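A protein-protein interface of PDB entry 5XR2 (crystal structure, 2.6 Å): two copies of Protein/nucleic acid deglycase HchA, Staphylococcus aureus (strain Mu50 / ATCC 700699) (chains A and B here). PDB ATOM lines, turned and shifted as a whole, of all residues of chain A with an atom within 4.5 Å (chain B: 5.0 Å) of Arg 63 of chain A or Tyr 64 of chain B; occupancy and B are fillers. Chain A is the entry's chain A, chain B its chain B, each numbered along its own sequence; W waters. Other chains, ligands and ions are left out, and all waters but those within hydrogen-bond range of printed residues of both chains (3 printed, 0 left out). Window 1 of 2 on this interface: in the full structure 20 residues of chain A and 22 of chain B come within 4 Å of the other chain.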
ATOM      1  N   ASP A  15       3.729 -21.371   1.685  1.00  0.00           N
ATOM      2  CA  ASP A  15       4.285 -20.537   0.601  1.00  0.00           C
ATOM      3  C   ASP A  15       4.893 -19.264   1.230  1.00  0.00           C
ATOM      4  O   ASP A  15       4.192 -18.329   1.587  1.00  0.00           O
ATOM      5  CB  ASP A  15       3.189 -20.244  -0.457  1.00  0.00           C
ATOM      6  CG  ASP A  15       3.695 -19.416  -1.695  1.00  0.00           C
ATOM      7  OD1 ASP A  15       4.861 -18.941  -1.712  1.00  0.00           O
ATOM      8  OD2 ASP A  15       2.898 -19.226  -2.661  1.00  0.00           O
ATOM      9  N   ALA A  17       6.283 -16.694   0.102  1.00  0.00           N
ATOM     10  CA  ALA A  17       5.966 -15.434  -0.555  1.00  0.00           C
ATOM     11  C   ALA A  17       4.749 -14.672  -0.016  1.00  0.00           C
ATOM     12  O   ALA A  17       4.623 -13.487  -0.276  1.00  0.00           O
ATOM     13  CB  ALA A  17       5.786 -15.656  -2.064  1.00  0.00           C
ATOM     14  N   GLU A  61      -3.928 -14.151 -13.657  1.00  0.00           N
ATOM     15  CA  GLU A  61      -2.804 -13.300 -13.226  1.00  0.00           C
ATOM     16  C   GLU A  61      -2.732 -13.172 -11.700  1.00  0.00           C
ATOM     17  O   GLU A  61      -1.782 -12.600 -11.178  1.00  0.00           O
ATOM     18  CB  GLU A  61      -2.853 -11.906 -13.913  1.00  0.00           C
ATOM     19  CG  GLU A  61      -3.975 -11.016 -13.386  1.00  0.00           C
ATOM     20  CD  GLU A  61      -4.191  -9.685 -14.111  1.00  0.00           C
ATOM     21  OE1 GLU A  61      -3.334  -9.234 -14.926  1.00  0.00           O
ATOM     22  OE2 GLU A  61      -5.258  -9.073 -13.811  1.00  0.00           O
ATOM     23  N   GLU A  62      -3.699 -13.730 -10.989  1.00  0.00           N
ATOM     24  CA  GLU A  62      -3.633 -13.842  -9.539  1.00  0.00           C
ATOM     25  C   GLU A  62      -3.392 -15.300  -9.177  1.00  0.00           C
ATOM     26  O   GLU A  62      -4.061 -16.155  -9.668  1.00  0.00           O
ATOM     27  CB  GLU A  62      -4.927 -13.356  -8.932  1.00  0.00           C
ATOM     28  CG  GLU A  62      -5.008 -13.454  -7.415  1.00  0.00           C
ATOM     29  CD  GLU A  62      -3.875 -12.725  -6.738  1.00  0.00           C
ATOM     30  OE1 GLU A  62      -3.233 -13.328  -5.835  1.00  0.00           O
ATOM     31  OE2 GLU A  62      -3.623 -11.579  -7.154  1.00  0.00           O
ATOM     32  N   ARG A  63      -2.427 -15.554  -8.306  1.00  0.00           N
ATOM     33  CA  ARG A  63      -2.096 -16.886  -7.813  1.00  0.00           C
ATOM     34  C   ARG A  63      -2.864 -17.269  -6.522  1.00  0.00           C
ATOM     35  O   ARG A  63      -3.016 -18.447  -6.257  1.00  0.00           O
ATOM     36  CB  ARG A  63      -0.572 -16.959  -7.607  1.00  0.00           C
ATOM     37  CG  ARG A  63      -0.068 -18.033  -6.664  1.00  0.00           C
ATOM     38  CD  ARG A  63       1.439 -18.176  -6.760  1.00  0.00           C
ATOM     39  NE  ARG A  63       1.808 -18.563  -8.118  1.00  0.00           N
ATOM     40  CZ  ARG A  63       2.639 -17.922  -8.936  1.00  0.00           C
ATOM     41  NH1 ARG A  63       3.296 -16.825  -8.533  1.00  0.00           N
ATOM     42  NH2 ARG A  63       2.852 -18.414 -10.179  1.00  0.00           N
ATOM     43  N   TYR A  64      -3.326 -16.310  -5.717  1.00  0.00           N
ATOM     44  CA  TYR A  64      -3.924 -16.641  -4.380  1.00  0.00           C
ATOM     45  C   TYR A  64      -5.445 -16.575  -4.322  1.00  0.00           C
ATOM     46  O   TYR A  64      -6.037 -15.561  -4.647  1.00  0.00           O
ATOM     47  CB  TYR A  64      -3.284 -15.814  -3.233  1.00  0.00           C
ATOM     48  CG  TYR A  64      -1.797 -16.032  -3.241  1.00  0.00           C
ATOM     49  CD1 TYR A  64      -1.245 -17.157  -2.644  1.00  0.00           C
ATOM     50  CD2 TYR A  64      -0.944 -15.157  -3.934  1.00  0.00           C
ATOM     51  CE1 TYR A  64       0.123 -17.388  -2.712  1.00  0.00           C
ATOM     52  CE2 TYR A  64       0.430 -15.371  -3.993  1.00  0.00           C
ATOM     53  CZ  TYR A  64       0.961 -16.499  -3.402  1.00  0.00           C
ATOM     54  OH  TYR A  64       2.303 -16.745  -3.459  1.00  0.00           O
ATOM     55  N   VAL A  65      -6.043 -17.703  -3.940  1.00  0.00           N
ATOM     56  CA  VAL A  65      -7.476 -17.811  -3.715  1.00  0.00           C
ATOM     57  C   VAL A  65      -7.765 -17.772  -2.208  1.00  0.00           C
ATOM     58  O   VAL A  65      -7.251 -18.587  -1.465  1.00  0.00           O
ATOM     59  CB  VAL A  65      -8.044 -19.107  -4.317  1.00  0.00           C
ATOM     60  CG1 VAL A  65      -9.533 -19.182  -4.034  1.00  0.00           C
ATOM     61  CG2 VAL A  65      -7.805 -19.145  -5.823  1.00  0.00           C
ATOM     62  N   PHE A  73      -4.992 -20.372  -0.939  1.00  0.00           N
ATOM     63  CA  PHE A  73      -4.477 -21.431  -1.805  1.00  0.00           C
ATOM     64  C   PHE A  73      -3.508 -20.805  -2.781  1.00  0.00           C
ATOM     65  O   PHE A  73      -3.883 -19.934  -3.539  1.00  0.00           O
ATOM     66  CB  PHE A  73      -5.627 -22.160  -2.534  1.00  0.00           C
ATOM     67  CG  PHE A  73      -5.196 -23.356  -3.341  1.00  0.00           C
ATOM     68  CD1 PHE A  73      -4.127 -24.173  -2.944  1.00  0.00           C
ATOM     69  CD2 PHE A  73      -5.874 -23.692  -4.507  1.00  0.00           C
ATOM     70  CE1 PHE A  73      -3.742 -25.283  -3.716  1.00  0.00           C
ATOM     71  CE2 PHE A  73      -5.495 -24.810  -5.273  1.00  0.00           C
ATOM     72  CZ  PHE A  73      -4.423 -25.605  -4.874  1.00  0.00           C
ATOM     73  N   SER A  74      -2.257 -21.224  -2.735  1.00  0.00           N
ATOM     74  CA  SER A  74      -1.272 -20.851  -3.756  1.00  0.00           C
ATOM     75  C   SER A  74      -1.499 -21.732  -4.968  1.00  0.00           C
ATOM     76  O   SER A  74      -1.186 -22.913  -4.929  1.00  0.00           O
ATOM     77  CB  SER A  74       0.135 -21.081  -3.247  1.00  0.00           C
ATOM     78  OG  SER A  74       1.071 -20.957  -4.300  1.00  0.00           O
ATOM     79  N   THR A  75      -2.025 -21.156  -6.040  1.00  0.00           N
ATOM     80  CA  THR A  75      -2.401 -21.913  -7.226  1.00  0.00           C
ATOM     81  C   THR A  75      -1.847 -21.265  -8.490  1.00  0.00           C
ATOM     82  O   THR A  75      -0.633 -21.140  -8.600  1.00  0.00           O
ATOM     83  CB  THR A  75      -3.945 -22.199  -7.271  1.00  0.00           C
ATOM     84  OG1 THR A  75      -4.376 -22.467  -8.612  1.00  0.00           O
ATOM     85  CG2 THR A  75      -4.798 -21.048  -6.724  1.00  0.00           C
ATOM     86  N   GLY A  76      -2.722 -20.922  -9.437  1.00  0.00           N
ATOM     87  CA  GLY A  76      -2.379 -20.351 -10.744  1.00  0.00           C
ATOM     88  C   GLY A  76      -3.146 -21.115 -11.799  1.00  0.00           C
ATOM     89  O   GLY A  76      -3.999 -21.908 -11.450  1.00  0.00           O
ATOM     90  N   LYS A 107       0.248 -16.410 -13.882  1.00  0.00           N
ATOM     91  CA  LYS A 107       0.545 -17.213 -12.718  1.00  0.00           C
ATOM     92  C   LYS A 107       0.208 -18.672 -13.027  1.00  0.00           C
ATOM     93  O   LYS A 107      -0.943 -18.999 -13.226  1.00  0.00           O
ATOM     94  CB  LYS A 107      -0.258 -16.704 -11.535  1.00  0.00           C
ATOM     95  CG  LYS A 107      -0.065 -15.221 -11.262  1.00  0.00           C
ATOM     96  CD  LYS A 107       1.372 -14.871 -10.935  1.00  0.00           C
ATOM     97  CE  LYS A 107       1.536 -13.388 -10.665  1.00  0.00           C
ATOM     98  NZ  LYS A 107       1.101 -12.514 -11.786  1.00  0.00           N
ATOM     99  N   LEU A 108       1.228 -19.529 -13.098  1.00  0.00           N
ATOM    100  CA  LEU A 108       1.043 -20.965 -13.266  1.00  0.00           C
ATOM    101  C   LEU A 108       1.190 -21.712 -11.934  1.00  0.00           C
ATOM    102  O   LEU A 108       1.860 -21.244 -11.007  1.00  0.00           O
ATOM    103  CB  LEU A 108       2.061 -21.508 -14.270  1.00  0.00           C
ATOM    104  CG  LEU A 108       1.996 -20.994 -15.712  1.00  0.00           C
ATOM    105  CD1 LEU A 108       3.248 -21.387 -16.473  1.00  0.00           C
ATOM    106  CD2 LEU A 108       0.793 -21.539 -16.448  1.00  0.00           C
ATOM    107  N   ASP B  15      12.395 -17.725  -5.397  1.00  0.00           N
ATOM    108  CA  ASP B  15      10.975 -17.833  -4.979  1.00  0.00           C
ATOM    109  C   ASP B  15      10.393 -19.043  -5.718  1.00  0.00           C
ATOM    110  O   ASP B  15      10.263 -19.010  -6.944  1.00  0.00           O
ATOM    111  CB  ASP B  15      10.219 -16.529  -5.337  1.00  0.00           C
ATOM    112  CG  ASP B  15       8.764 -16.468  -4.793  1.00  0.00           C
ATOM    113  OD1 ASP B  15       8.184 -17.471  -4.316  1.00  0.00           O
ATOM    114  OD2 ASP B  15       8.184 -15.366  -4.859  1.00  0.00           O
ATOM    115  N   ALA B  17       7.455 -20.358  -5.817  1.00  0.00           N
ATOM    116  CA  ALA B  17       6.124 -20.130  -6.412  1.00  0.00           C
ATOM    117  C   ALA B  17       6.169 -19.653  -7.838  1.00  0.00           C
ATOM    118  O   ALA B  17       5.170 -19.796  -8.532  1.00  0.00           O
ATOM    119  CB  ALA B  17       5.303 -19.161  -5.574  1.00  0.00           C
ATOM    120  N   GLU B  18       7.306 -19.116  -8.287  1.00  0.00           N
ATOM    121  CA  GLU B  18       7.400 -18.461  -9.593  1.00  0.00           C
ATOM    122  C   GLU B  18       8.640 -18.867 -10.403  1.00  0.00           C
ATOM    123  O   GLU B  18       9.644 -19.327  -9.839  1.00  0.00           O
ATOM    124  CB  GLU B  18       7.307 -16.932  -9.403  1.00  0.00           C
ATOM    125  CG  GLU B  18       7.021 -16.114 -10.668  1.00  0.00           C
ATOM    126  CD  GLU B  18       5.891 -16.682 -11.513  1.00  0.00           C
ATOM    127  OE1 GLU B  18       4.701 -16.573 -11.095  1.00  0.00           O
ATOM    128  OE2 GLU B  18       6.217 -17.273 -12.587  1.00  0.00           O
ATOM    129  N   ALA B  21      12.387 -16.154 -10.565  1.00  0.00           N
ATOM    130  CA  ALA B  21      12.030 -15.048  -9.673  1.00  0.00           C
ATOM    131  C   ALA B  21      12.748 -15.189  -8.340  1.00  0.00           C
ATOM    132  O   ALA B  21      12.923 -16.296  -7.825  1.00  0.00           O
ATOM    133  CB  ALA B  21      10.538 -15.022  -9.438  1.00  0.00           C
ATOM    134  N   GLU B  62       0.387  -6.848  -7.707  1.00  0.00           N
ATOM    135  CA  GLU B  62       1.315  -7.710  -8.444  1.00  0.00           C
ATOM    136  C   GLU B  62       2.672  -7.770  -7.749  1.00  0.00           C
ATOM    137  O   GLU B  62       3.362  -6.792  -7.674  1.00  0.00           O
ATOM    138  CB  GLU B  62       1.537  -7.187  -9.893  1.00  0.00           C
ATOM    139  CG  GLU B  62       2.470  -8.044 -10.776  1.00  0.00           C
ATOM    140  CD  GLU B  62       2.161  -9.531 -10.646  1.00  0.00           C
ATOM    141  OE1 GLU B  62       2.987 -10.283 -10.078  1.00  0.00           O
ATOM    142  OE2 GLU B  62       1.049  -9.951 -11.023  1.00  0.00           O
ATOM    143  N   ARG B  63       3.085  -8.942  -7.323  1.00  0.00           N
ATOM    144  CA  ARG B  63       4.362  -9.125  -6.608  1.00  0.00           C
ATOM    145  C   ARG B  63       5.649  -9.071  -7.488  1.00  0.00           C
ATOM    146  O   ARG B  63       6.725  -8.703  -6.994  1.00  0.00           O
ATOM    147  CB  ARG B  63       4.269 -10.443  -5.818  1.00  0.00           C
ATOM    148  CG  ARG B  63       5.568 -11.033  -5.351  1.00  0.00           C
ATOM    149  CD  ARG B  63       5.345 -12.039  -4.262  1.00  0.00           C
ATOM    150  NE  ARG B  63       4.930 -11.394  -3.008  1.00  0.00           N
ATOM    151  CZ  ARG B  63       3.781 -11.603  -2.366  1.00  0.00           C
ATOM    152  NH1 ARG B  63       2.842 -12.431  -2.829  1.00  0.00           N
ATOM    153  NH2 ARG B  63       3.562 -10.958  -1.225  1.00  0.00           N
ATOM    154  N   TYR B  64       5.539  -9.420  -8.768  1.00  0.00           N
ATOM    155  CA  TYR B  64       6.718  -9.722  -9.604  1.00  0.00           C
ATOM    156  C   TYR B  64       7.010  -8.608 -10.580  1.00  0.00           C
ATOM    157  O   TYR B  64       6.109  -8.147 -11.306  1.00  0.00           O
ATOM    158  CB  TYR B  64       6.559 -11.097 -10.312  1.00  0.00           C
ATOM    159  CG  TYR B  64       6.439 -12.221  -9.274  1.00  0.00           C
ATOM    160  CD1 TYR B  64       7.521 -12.588  -8.506  1.00  0.00           C
ATOM    161  CD2 TYR B  64       5.221 -12.846  -9.006  1.00  0.00           C
ATOM    162  CE1 TYR B  64       7.412 -13.567  -7.539  1.00  0.00           C
ATOM    163  CE2 TYR B  64       5.116 -13.823  -8.050  1.00  0.00           C
ATOM    164  CZ  TYR B  64       6.215 -14.177  -7.320  1.00  0.00           C
ATOM    165  OH  TYR B  64       6.141 -15.130  -6.353  1.00  0.00           O
ATOM    166  N   VAL B  65       8.269  -8.152 -10.563  1.00  0.00           N
ATOM    167  CA  VAL B  65       8.738  -7.087 -11.449  1.00  0.00           C
ATOM    168  C   VAL B  65       9.693  -7.738 -12.445  1.00  0.00           C
ATOM    169  O   VAL B  65      10.692  -8.304 -12.048  1.00  0.00           O
ATOM    170  CB  VAL B  65       9.461  -5.966 -10.653  1.00  0.00           C
ATOM    171  CG1 VAL B  65       9.995  -4.885 -11.577  1.00  0.00           C
ATOM    172  CG2 VAL B  65       8.544  -5.337  -9.629  1.00  0.00           C
ATOM    173  N   LEU B  66       9.375  -7.671 -13.733  1.00  0.00           N
ATOM    174  CA  LEU B  66      10.267  -8.180 -14.781  1.00  0.00           C
ATOM    175  C   LEU B  66      11.460  -7.233 -14.948  1.00  0.00           C
ATOM    176  O   LEU B  66      11.278  -6.005 -15.055  1.00  0.00           O
ATOM    177  CB  LEU B  66       9.505  -8.326 -16.092  1.00  0.00           C
ATOM    178  CG  LEU B  66      10.199  -8.983 -17.286  1.00  0.00           C
ATOM    179  CD1 LEU B  66      10.679 -10.412 -17.010  1.00  0.00           C
ATOM    180  CD2 LEU B  66       9.271  -8.995 -18.482  1.00  0.00           C
ATOM    181  N   MET B  72      12.955 -12.114 -12.397  1.00  0.00           N
ATOM    182  CA  MET B  72      11.879 -11.302 -11.785  1.00  0.00           C
ATOM    183  C   MET B  72      12.184 -11.018 -10.358  1.00  0.00           C
ATOM    184  O   MET B  72      12.737 -11.880  -9.656  1.00  0.00           O
ATOM    185  CB  MET B  72      10.499 -11.969 -11.903  1.00  0.00           C
ATOM    186  CG  MET B  72      10.018 -11.958 -13.338  1.00  0.00           C
ATOM    187  SD  MET B  72       8.277 -12.194 -13.591  1.00  0.00           S
ATOM    188  CE  MET B  72       8.136 -13.791 -12.826  1.00  0.00           C
ATOM    189  N   PHE B  73      11.819  -9.824  -9.911  1.00  0.00           N
ATOM    190  CA  PHE B  73      12.049  -9.487  -8.511  1.00  0.00           C
ATOM    191  C   PHE B  73      10.780  -9.790  -7.705  1.00  0.00           C
ATOM    192  O   PHE B  73       9.718  -9.291  -8.042  1.00  0.00           O
ATOM    193  CB  PHE B  73      12.501  -8.035  -8.390  1.00  0.00           C
ATOM    194  CG  PHE B  73      12.801  -7.615  -6.985  1.00  0.00           C
ATOM    195  CD1 PHE B  73      13.622  -8.402  -6.156  1.00  0.00           C
ATOM    196  CD2 PHE B  73      12.295  -6.407  -6.482  1.00  0.00           C
ATOM    197  CE1 PHE B  73      13.892  -8.014  -4.855  1.00  0.00           C
ATOM    198  CE2 PHE B  73      12.585  -6.017  -5.178  1.00  0.00           C
ATOM    199  CZ  PHE B  73      13.370  -6.822  -4.363  1.00  0.00           C
ATOM    200  N   SER B  74      10.889 -10.652  -6.694  1.00  0.00           N
ATOM    201  CA  SER B  74       9.784 -10.966  -5.821  1.00  0.00           C
ATOM    202  C   SER B  74       9.669  -9.917  -4.716  1.00  0.00           C
ATOM    203  O   SER B  74      10.274 -10.034  -3.645  1.00  0.00           O
ATOM    204  CB  SER B  74       9.925 -12.340  -5.188  1.00  0.00           C
ATOM    205  OG  SER B  74       8.880 -12.557  -4.246  1.00  0.00           O
ATOM    206  N   VAL B 164       4.716  -1.203 -10.856  1.00  0.00           N
ATOM    207  CA  VAL B 164       3.942  -2.025 -11.835  1.00  0.00           C
ATOM    208  C   VAL B 164       2.424  -1.789 -11.815  1.00  0.00           C
ATOM    209  O   VAL B 164       1.823  -1.844 -10.753  1.00  0.00           O
ATOM    210  CB  VAL B 164       4.085  -3.548 -11.552  1.00  0.00           C
ATOM    211  CG1 VAL B 164       3.542  -4.355 -12.717  1.00  0.00           C
ATOM    212  CG2 VAL B 164       5.521  -3.944 -11.273  1.00  0.00           C
HETATM  213  O   HOH W   1       3.890 -18.348 -13.316  1.00  0.00           O
HETATM  214  O   HOH W   2       3.579 -22.029  -8.370  1.00  0.00           O
HETATM  215  O   HOH W   3       7.339 -18.989  -2.015  1.00  0.00           O
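NH2 of Arg 63 of chain B is in hydrogen-bond range of O of Ala 17 of chain A (2.9 Å).
NH2 of Arg 63 of chain A is in hydrogen-bond range of O of Ala 17 of chain B (3.2 Å).
The guanidinium group (NH2) of Arg 63 of chain A is in salt-bridge range of the side-chain carboxylate (OE1) of Glu 18 of chain B (2.8 Å).
NZ of Lys 107 of chain A lies within salt-bridge range of OE2 of Glu 62 of chain B, 2.7 Å away.
N of Ala 17 of chain A sits close to OD1 of Asp 15 of chain A (3.2 Å).
OD2 of Asp 15 of chain A lies within hydrogen-bond range of OG of Ser 74 of chain A.
O of Glu 61 of chain A is in hydrogen-bond range of NZ of Lys 107 of chain A (2.9 Å).
The backbone carbonyl oxygen (O) of Leu 108 of chain A sits at hydrogen-bond distance from the guanidinium group (NH2) of Arg 63 of chain A (3.1 Å).
OD1 of Asp 15 of chain B lies close to N of Ala 17 of chain B (3.3 Å).
The backbone NH (N) of Tyr 64 of chain B is in hydrogen-bond range of the side-chain carboxylate (OE1) of Glu 62 of chain B, 3.0 Å away.
Among the printed residues, merely in contact across the chains: Arg 63 of chain A with Tyr 64 of chain B (3.5 Å), Ala 17 of chain A with Asp 15 of chain B (3.7 Å), Lys 107 of chain A with Glu 18 of chain B (3.7 Å), Asp 15 of chain A with Ala 17 of chain B (3.8 Å), Glu 61 of chain A with Glu 62 of chain B (3.9 Å) and Tyr 64 of chain A with Arg 63 of chain B (3.98 Å).
Of chain B, only Ala 17 (3.2 Å), Glu 18 (2.8 Å) and Tyr 64 (3.5 Å) come within 4 Å of Arg 63 of chain A.
Of the printed residues of chain B, Tyr 64 of chain A touches Arg 63.
Printed residues of chain B within 4 Å of Lys 107 of chain A: Glu 18 (3.7 Å) and Glu 62 (2.7 Å).
Of chain A, only Arg 63 (3.5 Å) comes within 4 Å of Tyr 64 of chain B.
The nearest printed residue of chain B that does not touch Arg 63 of chain A is Asp 15 of chain B (6.3 Å).
Among the printed residues, Asp or Glu carboxylates within 4 Å of a Lys or Arg side-chain nitrogen of the other chain: Arg 63 of chain A with Glu 18 of chain B (2.8 Å) and Lys 107 of chain A with Glu 62 of chain B (2.7 Å).
Asp 15 of chain A touches Ala 17 of chain B, and with the chains exchanged Ala 17 of chain A touches Asp 15 of chain B.
Ala 17 of chain A touches Arg 63 of chain B, and with the chains exchanged Arg 63 of chain A touches Ala 17 of chain B.
Arg 63 of chain A touches Tyr 64 of chain B, and with the chains exchanged Tyr 64 of chain A touches Arg 63 of chain B.
Positions printed for both chains: 15, 17, 62, 63, 64, 65, 73 and 74.
Water W3 lies within hydrogen-bond range of the side-chain carboxylate (OD1) of Asp 15 of chain A, the side-chain carboxylate (OD1) of Asp 15 of chain B and the backbone NH (N) of Ala 17 of chain A.
Water W1 lies within hydrogen-bond range of OE2 of Glu 18 of chain B, N of Leu 108 of chain A and NH2 of Arg 63 of chain A.
Water W2 bridges O of Ala 17 of chain B and O of Leu 108 of chain A.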
